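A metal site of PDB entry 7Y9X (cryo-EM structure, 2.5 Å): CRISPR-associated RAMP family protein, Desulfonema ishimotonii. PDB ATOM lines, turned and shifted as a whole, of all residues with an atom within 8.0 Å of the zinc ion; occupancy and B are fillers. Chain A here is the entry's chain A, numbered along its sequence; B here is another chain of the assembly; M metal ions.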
ATOM      1  N   ARG A 452     -21.678  32.358  -5.529  1.00  0.00           N
ATOM      2  CA  ARG A 452     -22.691  31.594  -6.259  1.00  0.00           C
ATOM      3  C   ARG A 452     -22.575  31.821  -7.754  1.00  0.00           C
ATOM      4  O   ARG A 452     -22.685  30.872  -8.545  1.00  0.00           O
ATOM      5  CB  ARG A 452     -24.095  31.976  -5.762  1.00  0.00           C
ATOM      6  CG  ARG A 452     -25.208  31.226  -6.448  1.00  0.00           C
ATOM      7  CD  ARG A 452     -26.567  31.618  -5.911  1.00  0.00           C
ATOM      8  NE  ARG A 452     -26.721  31.317  -4.491  1.00  0.00           N
ATOM      9  CZ  ARG A 452     -27.122  30.146  -4.022  1.00  0.00           C
ATOM     10  NH1 ARG A 452     -27.388  29.127  -4.826  1.00  0.00           N
ATOM     11  NH2 ARG A 452     -27.282  29.990  -2.710  1.00  0.00           N
ATOM     12  N   GLN A 456     -21.320  28.799 -10.462  1.00  0.00           N
ATOM     13  CA  GLN A 456     -22.052  28.495 -11.686  1.00  0.00           C
ATOM     14  C   GLN A 456     -21.197  28.727 -12.918  1.00  0.00           C
ATOM     15  O   GLN A 456     -21.404  28.064 -13.935  1.00  0.00           O
ATOM     16  CB  GLN A 456     -23.320  29.333 -11.765  1.00  0.00           C
ATOM     17  CG  GLN A 456     -24.290  29.096 -10.629  1.00  0.00           C
ATOM     18  CD  GLN A 456     -25.522  29.959 -10.744  1.00  0.00           C
ATOM     19  OE1 GLN A 456     -26.178  29.972 -11.773  1.00  0.00           O
ATOM     20  NE2 GLN A 456     -25.817  30.686  -9.688  1.00  0.00           N
ATOM     21  N   SER A 461     -23.034  25.890 -15.558  1.00  0.00           N
ATOM     22  CA  SER A 461     -24.401  25.400 -15.402  1.00  0.00           C
ATOM     23  C   SER A 461     -25.225  26.432 -14.648  1.00  0.00           C
ATOM     24  O   SER A 461     -25.099  26.562 -13.424  1.00  0.00           O
ATOM     25  CB  SER A 461     -24.427  24.061 -14.672  1.00  0.00           C
ATOM     26  OG  SER A 461     -23.688  23.076 -15.368  1.00  0.00           O
ATOM     27  N   PRO A 462     -26.075  27.185 -15.348  1.00  0.00           N
ATOM     28  CA  PRO A 462     -27.008  28.070 -14.656  1.00  0.00           C
ATOM     29  C   PRO A 462     -27.959  27.275 -13.771  1.00  0.00           C
ATOM     30  O   PRO A 462     -28.349  26.155 -14.094  1.00  0.00           O
ATOM     31  CB  PRO A 462     -27.764  28.751 -15.794  1.00  0.00           C
ATOM     32  CG  PRO A 462     -26.794  28.726 -16.916  1.00  0.00           C
ATOM     33  CD  PRO A 462     -26.138  27.373 -16.805  1.00  0.00           C
ATOM     34  N   CYS A 463     -28.326  27.869 -12.643  1.00  0.00           N
ATOM     35  CA  CYS A 463     -29.339  27.322 -11.765  1.00  0.00           C
ATOM     36  C   CYS A 463     -30.658  28.055 -12.020  1.00  0.00           C
ATOM     37  O   CYS A 463     -30.701  29.280 -11.969  1.00  0.00           O
ATOM     38  CB  CYS A 463     -28.939  27.463 -10.306  1.00  0.00           C
ATOM     39  SG  CYS A 463     -30.108  26.727  -9.157  1.00  0.00           S
ATOM     40  N   ASN A 464     -31.712  27.288 -12.296  1.00  0.00           N
ATOM     41  CA  ASN A 464     -33.028  27.859 -12.555  1.00  0.00           C
ATOM     42  C   ASN A 464     -33.981  27.635 -11.394  1.00  0.00           C
ATOM     43  O   ASN A 464     -35.205  27.680 -11.579  1.00  0.00           O
ATOM     44  CB  ASN A 464     -33.616  27.276 -13.855  1.00  0.00           C
ATOM     45  CG  ASN A 464     -33.868  25.789 -13.765  1.00  0.00           C
ATOM     46  OD1 ASN A 464     -33.405  25.113 -12.859  1.00  0.00           O
ATOM     47  ND2 ASN A 464     -34.624  25.272 -14.725  1.00  0.00           N
ATOM     48  N   ALA A 465     -33.451  27.398 -10.197  1.00  0.00           N
ATOM     49  CA  ALA A 465     -34.305  27.191  -9.037  1.00  0.00           C
ATOM     50  C   ALA A 465     -35.068  28.455  -8.685  1.00  0.00           C
ATOM     51  O   ALA A 465     -34.590  29.581  -8.876  1.00  0.00           O
ATOM     52  CB  ALA A 465     -33.467  26.726  -7.839  1.00  0.00           C
ATOM     53  N   GLU A 466     -36.272  28.270  -8.166  1.00  0.00           N
ATOM     54  CA  GLU A 466     -37.126  29.355  -7.737  1.00  0.00           C
ATOM     55  C   GLU A 466     -37.094  29.457  -6.219  1.00  0.00           C
ATOM     56  O   GLU A 466     -36.737  28.511  -5.519  1.00  0.00           O
ATOM     57  CB  GLU A 466     -38.562  29.134  -8.220  1.00  0.00           C
ATOM     58  CG  GLU A 466     -38.697  29.060  -9.734  1.00  0.00           C
ATOM     59  CD  GLU A 466     -38.496  30.403 -10.398  1.00  0.00           C
ATOM     60  OE1 GLU A 466     -38.725  31.439  -9.733  1.00  0.00           O
ATOM     61  OE2 GLU A 466     -38.096  30.427 -11.570  1.00  0.00           O
ATOM     62  N   PRO A 471     -34.790  22.387  -1.154  1.00  0.00           N
ATOM     63  CA  PRO A 471     -33.545  22.999  -1.627  1.00  0.00           C
ATOM     64  C   PRO A 471     -33.071  22.374  -2.934  1.00  0.00           C
ATOM     65  O   PRO A 471     -33.173  21.165  -3.151  1.00  0.00           O
ATOM     66  CB  PRO A 471     -32.560  22.736  -0.491  1.00  0.00           C
ATOM     67  CG  PRO A 471     -33.401  22.554   0.699  1.00  0.00           C
ATOM     68  CD  PRO A 471     -34.656  21.896   0.229  1.00  0.00           C
ATOM     69  N   CYS A 472     -32.539  23.216  -3.808  1.00  0.00           N
ATOM     70  CA  CYS A 472     -32.057  22.743  -5.094  1.00  0.00           C
ATOM     71  C   CYS A 472     -30.821  21.875  -4.912  1.00  0.00           C
ATOM     72  O   CYS A 472     -29.987  22.115  -4.047  1.00  0.00           O
ATOM     73  CB  CYS A 472     -31.767  23.922  -6.020  1.00  0.00           C
ATOM     74  SG  CYS A 472     -30.891  23.457  -7.504  1.00  0.00           S
ATOM     75  N   MET A 473     -30.714  20.854  -5.766  1.00  0.00           N
ATOM     76  CA  MET A 473     -29.685  19.825  -5.631  1.00  0.00           C
ATOM     77  C   MET A 473     -28.605  19.925  -6.694  1.00  0.00           C
ATOM     78  O   MET A 473     -27.892  18.939  -6.922  1.00  0.00           O
ATOM     79  CB  MET A 473     -30.324  18.443  -5.648  1.00  0.00           C
ATOM     80  CG  MET A 473     -31.049  18.092  -4.377  1.00  0.00           C
ATOM     81  SD  MET A 473     -29.936  18.103  -2.956  1.00  0.00           S
ATOM     82  CE  MET A 473     -31.099  17.933  -1.626  1.00  0.00           C
ATOM     83  N   CYS A 474     -28.454  21.070  -7.351  1.00  0.00           N
ATOM     84  CA  CYS A 474     -27.339  21.209  -8.264  1.00  0.00           C
ATOM     85  C   CYS A 474     -26.045  21.384  -7.480  1.00  0.00           C
ATOM     86  O   CYS A 474     -26.030  21.624  -6.272  1.00  0.00           O
ATOM     87  CB  CYS A 474     -27.546  22.379  -9.228  1.00  0.00           C
ATOM     88  SG  CYS A 474     -27.392  24.044  -8.549  1.00  0.00           S
ATOM     89  N   LYS A 475     -24.927  21.264  -8.199  1.00  0.00           N
ATOM     90  CA  LYS A 475     -23.616  21.318  -7.575  1.00  0.00           C
ATOM     91  C   LYS A 475     -23.358  22.670  -6.933  1.00  0.00           C
ATOM     92  O   LYS A 475     -22.717  22.743  -5.874  1.00  0.00           O
ATOM     93  CB  LYS A 475     -22.549  20.992  -8.613  1.00  0.00           C
ATOM     94  CG  LYS A 475     -22.721  19.635  -9.272  1.00  0.00           C
ATOM     95  CD  LYS A 475     -21.746  19.454 -10.414  1.00  0.00           C
ATOM     96  CE  LYS A 475     -21.969  18.123 -11.107  1.00  0.00           C
ATOM     97  NZ  LYS A 475     -21.043  17.921 -12.257  1.00  0.00           N
ATOM     98  N   THR A 476     -23.829  23.753  -7.545  1.00  0.00           N
ATOM     99  CA  THR A 476     -23.633  25.080  -6.981  1.00  0.00           C
ATOM    100  C   THR A 476     -24.394  25.258  -5.671  1.00  0.00           C
ATOM    101  O   THR A 476     -23.842  25.752  -4.676  1.00  0.00           O
ATOM    102  CB  THR A 476     -24.045  26.155  -7.980  1.00  0.00           C
ATOM    103  OG1 THR A 476     -23.259  26.031  -9.173  1.00  0.00           O
ATOM    104  CG2 THR A 476     -23.843  27.539  -7.394  1.00  0.00           C
ATOM    105  N   CYS A 477     -25.669  24.858  -5.650  1.00  0.00           N
ATOM    106  CA  CYS A 477     -26.488  25.084  -4.466  1.00  0.00           C
ATOM    107  C   CYS A 477     -26.034  24.222  -3.295  1.00  0.00           C
ATOM    108  O   CYS A 477     -26.191  24.610  -2.139  1.00  0.00           O
ATOM    109  CB  CYS A 477     -27.964  24.810  -4.782  1.00  0.00           C
ATOM    110  SG  CYS A 477     -28.806  26.130  -5.671  1.00  0.00           S
ATOM    111  N   ARG A 478     -25.510  23.027  -3.575  1.00  0.00           N
ATOM    112  CA  ARG A 478     -25.045  22.173  -2.487  1.00  0.00           C
ATOM    113  C   ARG A 478     -23.736  22.677  -1.901  1.00  0.00           C
ATOM    114  O   ARG A 478     -23.491  22.525  -0.700  1.00  0.00           O
ATOM    115  CB  ARG A 478     -24.908  20.727  -2.976  1.00  0.00           C
ATOM    116  CG  ARG A 478     -26.252  20.056  -3.213  1.00  0.00           C
ATOM    117  CD  ARG A 478     -26.149  18.578  -3.525  1.00  0.00           C
ATOM    118  NE  ARG A 478     -25.708  18.310  -4.882  1.00  0.00           N
ATOM    119  CZ  ARG A 478     -24.515  17.834  -5.210  1.00  0.00           C
ATOM    120  NH1 ARG A 478     -23.613  17.538  -4.289  1.00  0.00           N
ATOM    121  NH2 ARG A 478     -24.227  17.634  -6.497  1.00  0.00           N
ATOM    122  N   ARG A 481     -24.545  25.767   0.271  1.00  0.00           N
ATOM    123  CA  ARG A 481     -25.102  25.422   1.570  1.00  0.00           C
ATOM    124  C   ARG A 481     -24.038  24.963   2.555  1.00  0.00           C
ATOM    125  O   ARG A 481     -24.361  24.782   3.733  1.00  0.00           O
ATOM    126  CB  ARG A 481     -26.183  24.355   1.420  1.00  0.00           C
ATOM    127  CG  ARG A 481     -27.476  24.866   0.825  1.00  0.00           C
ATOM    128  CD  ARG A 481     -28.639  23.921   1.070  1.00  0.00           C
ATOM    129  NE  ARG A 481     -28.499  22.666   0.338  1.00  0.00           N
ATOM    130  CZ  ARG A 481     -28.928  22.463  -0.893  1.00  0.00           C
ATOM    131  NH1 ARG A 481     -29.514  23.427  -1.588  1.00  0.00           N
ATOM    132  NH2 ARG A 481     -28.760  21.278  -1.454  1.00  0.00           N
ATOM    133  N   MET B 620     -29.967  22.317 -16.605  1.00  0.00           N
ATOM    134  CA  MET B 620     -31.323  22.316 -16.060  1.00  0.00           C
ATOM    135  C   MET B 620     -32.241  23.192 -16.889  1.00  0.00           C
ATOM    136  O   MET B 620     -33.410  22.843 -17.103  1.00  0.00           O
ATOM    137  CB  MET B 620     -31.317  22.800 -14.612  1.00  0.00           C
ATOM    138  CG  MET B 620     -30.409  22.035 -13.686  1.00  0.00           C
ATOM    139  SD  MET B 620     -30.452  22.726 -12.018  1.00  0.00           S
ATOM    140  CE  MET B 620     -30.261  21.231 -11.054  1.00  0.00           C
HETATM  141 ZN    ZN M   1     -29.283  25.106  -7.712  1.00  0.00          ZN
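NH1 of Arg 481 is in hydrogen-bond range of O of Cys 472, 2.8 Å away. The side-chain sulfur (SG) of Cys 463 sits close to the backbone NH (N) of Ala 465 (3.6 Å). N of Cys 463 sits at hydrogen-bond distance from OE1 of Gln 456 (3.1 Å). N of Thr 476 sits close to SG of Cys 474 (3.7 Å). The guanidinium group of Arg 452 lies close to the side-chain sulfur of Cys 477, 3.4 Å away.
Within 4 Å of the zinc ion: Cys 463, Cys 472, Cys 474 and Cys 477. The nearest printed residue that does not touch the zinc ion is Ala 465 (4.5 Å).
The zinc ion is bound by SG of Cys 472 (2.3 Å). The side-chain sulfur (SG) of Cys 463 is bound to the zinc ion, 2.3 Å away. SG of Cys 474 binds the zinc ion (2.3 Å). The side-chain sulfur (SG) of Cys 477 binds the zinc ion, 2.3 Å away.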
